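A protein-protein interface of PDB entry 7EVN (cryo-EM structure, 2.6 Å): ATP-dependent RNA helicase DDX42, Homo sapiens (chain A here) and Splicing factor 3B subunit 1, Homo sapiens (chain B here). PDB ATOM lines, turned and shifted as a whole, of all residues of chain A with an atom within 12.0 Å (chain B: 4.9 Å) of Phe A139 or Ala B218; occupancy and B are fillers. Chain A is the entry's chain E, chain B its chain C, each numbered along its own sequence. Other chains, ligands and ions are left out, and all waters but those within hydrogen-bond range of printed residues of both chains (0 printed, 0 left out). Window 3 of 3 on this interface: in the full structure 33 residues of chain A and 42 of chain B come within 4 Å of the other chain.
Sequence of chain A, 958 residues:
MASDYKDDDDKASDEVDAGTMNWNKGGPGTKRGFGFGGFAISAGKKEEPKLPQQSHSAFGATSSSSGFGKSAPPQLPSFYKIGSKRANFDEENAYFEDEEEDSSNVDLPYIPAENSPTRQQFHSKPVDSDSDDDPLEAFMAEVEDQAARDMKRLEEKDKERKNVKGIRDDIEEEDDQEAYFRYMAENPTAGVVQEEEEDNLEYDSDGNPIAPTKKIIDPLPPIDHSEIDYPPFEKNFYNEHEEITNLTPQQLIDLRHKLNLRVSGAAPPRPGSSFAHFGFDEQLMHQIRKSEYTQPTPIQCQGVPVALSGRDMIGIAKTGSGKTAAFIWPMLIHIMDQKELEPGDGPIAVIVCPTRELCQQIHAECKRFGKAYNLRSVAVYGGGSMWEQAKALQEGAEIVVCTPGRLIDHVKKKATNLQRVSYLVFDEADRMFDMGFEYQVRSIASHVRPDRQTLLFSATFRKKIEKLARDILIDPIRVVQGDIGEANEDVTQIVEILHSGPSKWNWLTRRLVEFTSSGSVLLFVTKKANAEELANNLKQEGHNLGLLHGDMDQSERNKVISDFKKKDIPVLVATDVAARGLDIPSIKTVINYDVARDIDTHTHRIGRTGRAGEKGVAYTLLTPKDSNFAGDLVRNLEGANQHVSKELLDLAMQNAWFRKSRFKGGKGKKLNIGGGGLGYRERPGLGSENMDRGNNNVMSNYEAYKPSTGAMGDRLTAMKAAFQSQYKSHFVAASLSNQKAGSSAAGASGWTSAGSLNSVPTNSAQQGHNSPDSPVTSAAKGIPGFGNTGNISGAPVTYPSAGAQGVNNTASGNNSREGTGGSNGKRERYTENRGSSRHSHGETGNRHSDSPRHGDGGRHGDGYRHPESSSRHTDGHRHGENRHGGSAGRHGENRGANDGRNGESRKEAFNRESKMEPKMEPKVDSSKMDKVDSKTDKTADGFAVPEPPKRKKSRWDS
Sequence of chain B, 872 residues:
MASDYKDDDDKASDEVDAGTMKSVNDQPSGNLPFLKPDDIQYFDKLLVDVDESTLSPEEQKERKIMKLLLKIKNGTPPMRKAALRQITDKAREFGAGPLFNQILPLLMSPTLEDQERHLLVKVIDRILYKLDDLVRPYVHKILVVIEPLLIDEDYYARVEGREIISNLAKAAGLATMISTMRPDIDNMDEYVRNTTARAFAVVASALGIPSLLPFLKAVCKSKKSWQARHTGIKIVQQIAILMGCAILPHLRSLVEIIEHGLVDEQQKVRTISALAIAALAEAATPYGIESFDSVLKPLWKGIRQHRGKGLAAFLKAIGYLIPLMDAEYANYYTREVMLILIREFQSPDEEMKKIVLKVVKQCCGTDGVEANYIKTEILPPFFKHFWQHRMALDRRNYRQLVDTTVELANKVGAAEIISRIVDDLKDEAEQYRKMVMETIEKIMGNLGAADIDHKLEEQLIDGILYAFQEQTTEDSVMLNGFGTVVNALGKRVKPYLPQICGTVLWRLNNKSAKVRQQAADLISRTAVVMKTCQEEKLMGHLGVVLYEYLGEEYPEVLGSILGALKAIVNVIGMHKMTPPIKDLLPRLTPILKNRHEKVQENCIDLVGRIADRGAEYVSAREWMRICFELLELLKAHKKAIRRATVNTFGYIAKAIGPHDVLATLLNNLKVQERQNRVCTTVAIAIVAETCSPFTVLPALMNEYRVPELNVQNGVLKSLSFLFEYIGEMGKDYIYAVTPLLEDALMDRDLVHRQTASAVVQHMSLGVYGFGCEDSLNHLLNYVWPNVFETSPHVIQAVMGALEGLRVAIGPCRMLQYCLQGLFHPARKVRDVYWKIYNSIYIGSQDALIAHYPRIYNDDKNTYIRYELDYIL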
ATOM      1  N   ASP A 134     -25.625 -10.534   1.847  1.00  0.00           N
ATOM      2  CA  ASP A 134     -25.368 -11.614   0.856  1.00  0.00           C
ATOM      3  C   ASP A 134     -23.945 -11.463   0.307  1.00  0.00           C
ATOM      4  O   ASP A 134     -23.159 -12.422   0.434  1.00  0.00           O
ATOM      5  CB  ASP A 134     -26.422 -11.612  -0.255  1.00  0.00           C
ATOM      6  CG  ASP A 134     -27.767 -12.158   0.192  1.00  0.00           C
ATOM      7  OD1 ASP A 134     -27.909 -12.449   1.396  1.00  0.00           O
ATOM      8  OD2 ASP A 134     -28.662 -12.293  -0.670  1.00  0.00           O
ATOM      9  N   PRO A 135     -23.574 -10.305  -0.283  1.00  0.00           N
ATOM     10  CA  PRO A 135     -22.225 -10.108  -0.816  1.00  0.00           C
ATOM     11  C   PRO A 135     -21.190 -10.183   0.316  1.00  0.00           C
ATOM     12  O   PRO A 135     -20.136 -10.756   0.106  1.00  0.00           O
ATOM     13  CB  PRO A 135     -22.265  -8.698  -1.424  1.00  0.00           C
ATOM     14  CG  PRO A 135     -23.421  -8.019  -0.722  1.00  0.00           C
ATOM     15  CD  PRO A 135     -24.420  -9.123  -0.451  1.00  0.00           C
ATOM     16  N   LEU A 136     -21.522  -9.607   1.475  1.00  0.00           N
ATOM     17  CA  LEU A 136     -20.604  -9.611   2.646  1.00  0.00           C
ATOM     18  C   LEU A 136     -20.644 -10.990   3.316  1.00  0.00           C
ATOM     19  O   LEU A 136     -19.769 -11.260   4.160  1.00  0.00           O
ATOM     20  CB  LEU A 136     -21.036  -8.513   3.622  1.00  0.00           C
ATOM     21  CG  LEU A 136     -19.904  -7.802   4.361  1.00  0.00           C
ATOM     22  CD1 LEU A 136     -20.455  -6.955   5.498  1.00  0.00           C
ATOM     23  CD2 LEU A 136     -18.886  -8.802   4.887  1.00  0.00           C
ATOM     24  N   GLU A 137     -21.633 -11.818   2.959  1.00  0.00           N
ATOM     25  CA  GLU A 137     -21.777 -13.180   3.539  1.00  0.00           C
ATOM     26  C   GLU A 137     -21.089 -14.214   2.636  1.00  0.00           C
ATOM     27  O   GLU A 137     -20.560 -15.201   3.176  1.00  0.00           O
ATOM     28  CB  GLU A 137     -23.253 -13.508   3.768  1.00  0.00           C
ATOM     29  CG  GLU A 137     -23.986 -12.451   4.576  1.00  0.00           C
ATOM     30  CD  GLU A 137     -23.205 -11.869   5.744  1.00  0.00           C
ATOM     31  OE1 GLU A 137     -22.170 -12.455   6.111  1.00  0.00           O
ATOM     32  OE2 GLU A 137     -23.639 -10.835   6.287  1.00  0.00           O
ATOM     33  N   ALA A 138     -21.101 -13.992   1.320  1.00  0.00           N
ATOM     34  CA  ALA A 138     -20.448 -14.928   0.374  1.00  0.00           C
ATOM     35  C   ALA A 138     -18.929 -14.749   0.444  1.00  0.00           C
ATOM     36  O   ALA A 138     -18.209 -15.620  -0.069  1.00  0.00           O
ATOM     37  CB  ALA A 138     -20.971 -14.704  -1.023  1.00  0.00           C
ATOM     38  N   PHE A 139     -18.475 -13.645   1.045  1.00  0.00           N
ATOM     39  CA  PHE A 139     -17.027 -13.357   1.209  1.00  0.00           C
ATOM     40  C   PHE A 139     -16.584 -13.800   2.607  1.00  0.00           C
ATOM     41  O   PHE A 139     -15.539 -14.454   2.725  1.00  0.00           O
ATOM     42  CB  PHE A 139     -16.743 -11.870   0.994  1.00  0.00           C
ATOM     43  CG  PHE A 139     -15.277 -11.534   0.915  1.00  0.00           C
ATOM     44  CD1 PHE A 139     -14.572 -11.162   2.047  1.00  0.00           C
ATOM     45  CD2 PHE A 139     -14.598 -11.613  -0.288  1.00  0.00           C
ATOM     46  CE1 PHE A 139     -13.222 -10.861   1.973  1.00  0.00           C
ATOM     47  CE2 PHE A 139     -13.246 -11.314  -0.361  1.00  0.00           C
ATOM     48  CZ  PHE A 139     -12.561 -10.938   0.770  1.00  0.00           C
ATOM     49  N   MET A 140     -17.404 -13.505   3.617  1.00  0.00           N
ATOM     50  CA  MET A 140     -17.085 -13.851   5.024  1.00  0.00           C
ATOM     51  C   MET A 140     -16.998 -15.371   5.165  1.00  0.00           C
ATOM     52  O   MET A 140     -16.059 -15.826   5.814  1.00  0.00           O
ATOM     53  CB  MET A 140     -18.143 -13.304   5.984  1.00  0.00           C
ATOM     54  CG  MET A 140     -17.818 -11.915   6.499  1.00  0.00           C
ATOM     55  SD  MET A 140     -16.106 -11.768   7.078  1.00  0.00           S
ATOM     56  CE  MET A 140     -15.231 -11.737   5.516  1.00  0.00           C
ATOM     57  N   ALA A 141     -17.883 -16.123   4.507  1.00  0.00           N
ATOM     58  CA  ALA A 141     -17.862 -17.604   4.596  1.00  0.00           C
ATOM     59  C   ALA A 141     -16.510 -18.160   4.121  1.00  0.00           C
ATOM     60  O   ALA A 141     -15.852 -18.889   4.901  1.00  0.00           O
ATOM     61  CB  ALA A 141     -18.999 -18.177   3.789  1.00  0.00           C
ATOM     62  N   GLU A 142     -16.111 -17.820   2.893  1.00  0.00           N
ATOM     63  CA  GLU A 142     -14.833 -18.313   2.307  1.00  0.00           C
ATOM     64  C   GLU A 142     -13.655 -17.816   3.149  1.00  0.00           C
ATOM     65  O   GLU A 142     -12.731 -18.614   3.402  1.00  0.00           O
ATOM     66  CB  GLU A 142     -14.693 -17.805   0.871  1.00  0.00           C
ATOM     67  CG  GLU A 142     -15.723 -18.385  -0.081  1.00  0.00           C
ATOM     68  CD  GLU A 142     -15.640 -17.844  -1.498  1.00  0.00           C
ATOM     69  OE1 GLU A 142     -15.651 -16.608  -1.660  1.00  0.00           O
ATOM     70  OE2 GLU A 142     -15.558 -18.663  -2.437  1.00  0.00           O
ATOM     71  N   VAL A 143     -13.707 -16.558   3.593  1.00  0.00           N
ATOM     72  CA  VAL A 143     -12.606 -15.984   4.423  1.00  0.00           C
ATOM     73  C   VAL A 143     -12.511 -16.785   5.724  1.00  0.00           C
ATOM     74  O   VAL A 143     -11.383 -17.127   6.118  1.00  0.00           O
ATOM     75  CB  VAL A 143     -12.847 -14.490   4.706  1.00  0.00           C
ATOM     76  CG1 VAL A 143     -12.052 -14.013   5.910  1.00  0.00           C
ATOM     77  CG2 VAL A 143     -12.550 -13.630   3.488  1.00  0.00           C
ATOM     78  N   GLU A 144     -13.656 -17.110   6.332  1.00  0.00           N
ATOM     79  CA  GLU A 144     -13.673 -17.891   7.598  1.00  0.00           C
ATOM     80  C   GLU A 144     -13.067 -19.275   7.345  1.00  0.00           C
ATOM     81  O   GLU A 144     -12.246 -19.719   8.172  1.00  0.00           O
ATOM     82  CB  GLU A 144     -15.101 -18.022   8.124  1.00  0.00           C
ATOM     83  CG  GLU A 144     -15.595 -16.784   8.851  1.00  0.00           C
ATOM     84  CD  GLU A 144     -16.968 -16.934   9.483  1.00  0.00           C
ATOM     85  OE1 GLU A 144     -17.477 -18.071   9.521  1.00  0.00           O
ATOM     86  OE2 GLU A 144     -17.525 -15.914   9.933  1.00  0.00           O
ATOM     87  N   ASP A 145     -13.485 -19.939   6.260  1.00  0.00           N
ATOM     88  CA  ASP A 145     -13.006 -21.308   5.916  1.00  0.00           C
ATOM     89  C   ASP A 145     -11.504 -21.293   5.613  1.00  0.00           C
ATOM     90  O   ASP A 145     -10.780 -22.148   6.165  1.00  0.00           O
ATOM     91  CB  ASP A 145     -13.811 -21.903   4.758  1.00  0.00           C
ATOM     92  CG  ASP A 145     -15.018 -22.705   5.216  1.00  0.00           C
ATOM     93  OD1 ASP A 145     -15.236 -22.794   6.441  1.00  0.00           O
ATOM     94  OD2 ASP A 145     -15.729 -23.243   4.342  1.00  0.00           O
ATOM     95  N   GLN A 146     -11.054 -20.346   4.788  1.00  0.00           N
ATOM     96  CA  GLN A 146      -9.615 -20.257   4.422  1.00  0.00           C
ATOM     97  C   GLN A 146      -8.805 -20.001   5.699  1.00  0.00           C
ATOM     98  O   GLN A 146      -7.771 -20.667   5.886  1.00  0.00           O
ATOM     99  CB  GLN A 146      -9.411 -19.114   3.425  1.00  0.00           C
ATOM    100  CG  GLN A 146      -8.532 -19.473   2.236  1.00  0.00           C
ATOM    101  CD  GLN A 146      -7.142 -19.903   2.632  1.00  0.00           C
ATOM    102  OE1 GLN A 146      -6.956 -20.778   3.471  1.00  0.00           O
ATOM    103  NE2 GLN A 146      -6.145 -19.294   2.009  1.00  0.00           N
ATOM    104  N   ALA A 147      -9.299 -19.111   6.566  1.00  0.00           N
ATOM    105  CA  ALA A 147      -8.593 -18.792   7.829  1.00  0.00           C
ATOM    106  C   ALA A 147      -8.509 -20.053   8.697  1.00  0.00           C
ATOM    107  O   ALA A 147      -7.420 -20.340   9.211  1.00  0.00           O
ATOM    108  CB  ALA A 147      -9.317 -17.682   8.548  1.00  0.00           C
ATOM    109  N   ALA A 148      -9.599 -20.818   8.792  1.00  0.00           N
ATOM    110  CA  ALA A 148      -9.580 -22.047   9.620  1.00  0.00           C
ATOM    111  C   ALA A 148      -8.546 -23.024   9.048  1.00  0.00           C
ATOM    112  O   ALA A 148      -7.756 -23.586   9.837  1.00  0.00           O
ATOM    113  CB  ALA A 148     -10.957 -22.661   9.648  1.00  0.00           C
ATOM    114  N   ARG A 149      -8.510 -23.162   7.718  1.00  0.00           N
ATOM    115  CA  ARG A 149      -7.547 -24.094   7.076  1.00  0.00           C
ATOM    116  C   ARG A 149      -6.111 -23.644   7.370  1.00  0.00           C
ATOM    117  O   ARG A 149      -5.285 -24.510   7.710  1.00  0.00           O
ATOM    118  CB  ARG A 149      -7.775 -24.129   5.563  1.00  0.00           C
ATOM    119  CG  ARG A 149      -9.074 -24.801   5.141  1.00  0.00           C
ATOM    120  CD  ARG A 149      -9.307 -24.600   3.656  1.00  0.00           C
ATOM    121  NE  ARG A 149      -8.055 -24.682   2.919  1.00  0.00           N
ATOM    122  CZ  ARG A 149      -7.584 -25.787   2.354  1.00  0.00           C
ATOM    123  NH1 ARG A 149      -8.269 -26.914   2.433  1.00  0.00           N
ATOM    124  NH2 ARG A 149      -6.432 -25.760   1.708  1.00  0.00           N
ATOM    125  N   ILE B 178      -8.440 -10.408   8.292  1.00  0.00           N
ATOM    126  CA  ILE B 178      -9.841 -10.149   7.979  1.00  0.00           C
ATOM    127  C   ILE B 178     -10.747 -10.840   8.990  1.00  0.00           C
ATOM    128  O   ILE B 178     -11.715 -10.254   9.485  1.00  0.00           O
ATOM    129  CB  ILE B 178     -10.161 -10.588   6.540  1.00  0.00           C
ATOM    130  CG1 ILE B 178      -9.481  -9.659   5.537  1.00  0.00           C
ATOM    131  CG2 ILE B 178     -11.653 -10.597   6.305  1.00  0.00           C
ATOM    132  CD1 ILE B 178      -9.755 -10.017   4.101  1.00  0.00           C
ATOM    133  N   PRO B 214     -11.427  -7.158  -3.150  1.00  0.00           N
ATOM    134  CA  PRO B 214     -12.671  -7.944  -3.060  1.00  0.00           C
ATOM    135  C   PRO B 214     -13.393  -7.812  -1.729  1.00  0.00           C
ATOM    136  O   PRO B 214     -14.631  -7.732  -1.716  1.00  0.00           O
ATOM    137  CB  PRO B 214     -12.201  -9.386  -3.307  1.00  0.00           C
ATOM    138  CG  PRO B 214     -10.745  -9.363  -3.127  1.00  0.00           C
ATOM    139  CD  PRO B 214     -10.290  -8.012  -3.527  1.00  0.00           C
ATOM    140  N   PHE B 215     -12.668  -7.786  -0.610  1.00  0.00           N
ATOM    141  CA  PHE B 215     -13.316  -7.583   0.680  1.00  0.00           C
ATOM    142  C   PHE B 215     -14.054  -6.252   0.711  1.00  0.00           C
ATOM    143  O   PHE B 215     -15.176  -6.161   1.217  1.00  0.00           O
ATOM    144  CB  PHE B 215     -12.285  -7.657   1.806  1.00  0.00           C
ATOM    145  CG  PHE B 215     -12.802  -7.191   3.136  1.00  0.00           C
ATOM    146  CD1 PHE B 215     -13.686  -7.964   3.862  1.00  0.00           C
ATOM    147  CD2 PHE B 215     -12.403  -5.978   3.660  1.00  0.00           C
ATOM    148  CE1 PHE B 215     -14.159  -7.536   5.082  1.00  0.00           C
ATOM    149  CE2 PHE B 215     -12.873  -5.544   4.877  1.00  0.00           C
ATOM    150  CZ  PHE B 215     -13.752  -6.325   5.590  1.00  0.00           C
ATOM    151  N   LEU B 216     -13.440  -5.206   0.158  1.00  0.00           N
ATOM    152  CA  LEU B 216     -14.081  -3.897   0.145  1.00  0.00           C
ATOM    153  C   LEU B 216     -15.274  -3.878  -0.798  1.00  0.00           C
ATOM    154  O   LEU B 216     -16.327  -3.319  -0.470  1.00  0.00           O
ATOM    155  CB  LEU B 216     -13.067  -2.828  -0.248  1.00  0.00           C
ATOM    156  CG  LEU B 216     -12.083  -2.447   0.850  1.00  0.00           C
ATOM    157  CD1 LEU B 216     -11.118  -1.403   0.340  1.00  0.00           C
ATOM    158  CD2 LEU B 216     -12.835  -1.950   2.059  1.00  0.00           C
ATOM    159  N   LYS B 217     -15.130  -4.494  -1.971  1.00  0.00           N
ATOM    160  CA  LYS B 217     -16.239  -4.595  -2.909  1.00  0.00           C
ATOM    161  C   LYS B 217     -17.437  -5.283  -2.279  1.00  0.00           C
ATOM    162  O   LYS B 217     -18.583  -4.941  -2.587  1.00  0.00           O
ATOM    163  CB  LYS B 217     -15.791  -5.345  -4.161  1.00  0.00           C
ATOM    164  CG  LYS B 217     -16.838  -5.434  -5.252  1.00  0.00           C
ATOM    165  CD  LYS B 217     -16.245  -6.008  -6.521  1.00  0.00           C
ATOM    166  CE  LYS B 217     -17.148  -5.773  -7.717  1.00  0.00           C
ATOM    167  NZ  LYS B 217     -18.404  -6.565  -7.651  1.00  0.00           N
ATOM    168  N   ALA B 218     -17.196  -6.245  -1.394  1.00  0.00           N
ATOM    169  CA  ALA B 218     -18.307  -6.902  -0.718  1.00  0.00           C
ATOM    170  C   ALA B 218     -18.850  -6.085   0.447  1.00  0.00           C
ATOM    171  O   ALA B 218     -20.068  -6.032   0.643  1.00  0.00           O
ATOM    172  CB  ALA B 218     -17.879  -8.281  -0.221  1.00  0.00           C
ATOM    173  N   VAL B 219     -17.978  -5.453   1.232  1.00  0.00           N
ATOM    174  CA  VAL B 219     -18.430  -4.828   2.470  1.00  0.00           C
ATOM    175  C   VAL B 219     -19.090  -3.482   2.201  1.00  0.00           C
ATOM    176  O   VAL B 219     -19.903  -3.017   3.005  1.00  0.00           O
ATOM    177  CB  VAL B 219     -17.258  -4.700   3.461  1.00  0.00           C
ATOM    178  CG1 VAL B 219     -16.349  -3.554   3.079  1.00  0.00           C
ATOM    179  CG2 VAL B 219     -17.766  -4.518   4.872  1.00  0.00           C
ATOM    180  N   CYS B 220     -18.776  -2.842   1.073  1.00  0.00           N
ATOM    181  CA  CYS B 220     -19.397  -1.564   0.749  1.00  0.00           C
ATOM    182  C   CYS B 220     -20.757  -1.733   0.085  1.00  0.00           C
ATOM    183  O   CYS B 220     -21.478  -0.745  -0.075  1.00  0.00           O
ATOM    184  CB  CYS B 220     -18.474  -0.746  -0.156  1.00  0.00           C
ATOM    185  SG  CYS B 220     -16.987  -0.135   0.653  1.00  0.00           S
ATOM    186  N   LYS B 221     -21.118  -2.953  -0.312  1.00  0.00           N
ATOM    187  CA  LYS B 221     -22.424  -3.247  -0.888  1.00  0.00           C
ATOM    188  C   LYS B 221     -23.280  -4.113   0.024  1.00  0.00           C
ATOM    189  O   LYS B 221     -24.252  -4.716  -0.440  1.00  0.00           O
ATOM    190  CB  LYS B 221     -22.268  -3.929  -2.248  1.00  0.00           C
ATOM    191  CG  LYS B 221     -22.112  -2.978  -3.419  1.00  0.00           C
ATOM    192  CD  LYS B 221     -23.465  -2.502  -3.912  1.00  0.00           C
ATOM    193  CE  LYS B 221     -23.395  -2.010  -5.347  1.00  0.00           C
ATOM    194  NZ  LYS B 221     -22.641  -2.956  -6.219  1.00  0.00           N
ATOM    195  N   SER B 222     -22.936  -4.198   1.305  1.00  0.00           N
ATOM    196  CA  SER B 222     -23.679  -5.048   2.223  1.00  0.00           C
ATOM    197  C   SER B 222     -25.098  -4.524   2.385  1.00  0.00           C
ATOM    198  O   SER B 222     -25.330  -3.313   2.344  1.00  0.00           O
ATOM    199  CB  SER B 222     -22.976  -5.113   3.575  1.00  0.00           C
ATOM    200  OG  SER B 222     -23.604  -4.262   4.514  1.00  0.00           O
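Ala B218 touches just these residues of chain A: Pro A135 (3.4 Å), Leu A136 (3.9 Å) and Phe A139 (3.96 Å). Of chain A, only Met A140 (3.8 Å) and Val A143 (3.5 Å) come within 4 Å of Ile B178. Pro B214 touches just one residue of chain A: Phe A139. Phe B215 touches just one residue of chain A: Phe A139 (3.3 Å). No residue of chain A comes within 4 Å of Lys B217. Lys B221 touches just one residue of chain A: Pro A135. Of chain A, only Leu A136 (3.7 Å) comes within 4 Å of Ser B222. Of the printed residues of chain B, Val A143 touches Ile B178. Of the printed residues of chain B, Met A140 touches Ile B178. Of the printed residues of chain B, Leu A136 touches Ala B218, Val B219 and Ser B222. Printed residues of chain B within 4 Å of Pro A135: Ala B218 and Lys B221. Gln A146 touches none of the printed residues of chain B. Ala A141 touches none of the printed residues of chain B. The nearest residue of chain A that does not touch Ala B218 is Glu A137 (6.1 Å). The nearest printed residue of chain B that does not touch Val A143 is Phe B215 (5.8 Å).
Printed residues of chain B that touch a printed residue of chain A: Ile B178, Pro B214, Phe B215, Ala B218, Val B219, Lys B221 and Ser B222. Along chain B the printed residues that touch a printed residue of chain A span positions 178 to 222. Of the 16 printed residues of chain A, 5 touch a printed residue of chain B. Printed residues of chain A that touch a printed residue of chain B: Pro A135, Leu A136, Phe A139, Met A140 and Val A143. Hydrophobic or aromatic side chains of chain A that line the printed part of chain B: Pro A135, Leu A136, Phe A139, Met A140 and Val A143. Among the printed residues, 10 pairs touch across the chains.
Among the printed residues, merely in contact across the chains: Pro A135 with Ala B218 (3.4 Å), Pro A135 with Lys B221 (3.4 Å), Leu A136 with Ala B218 (3.9 Å), Leu A136 with Val B219 (3.7 Å), Leu A136 with Ser B222 (3.7 Å), Phe A139 with Pro B214 (3.7 Å), Phe A139 with Phe B215 (3.3 Å), Phe A139 with Ala B218 (3.96 Å), Met A140 with Ile B178 (3.8 Å) and Val A143 with Ile B178 (3.5 Å).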
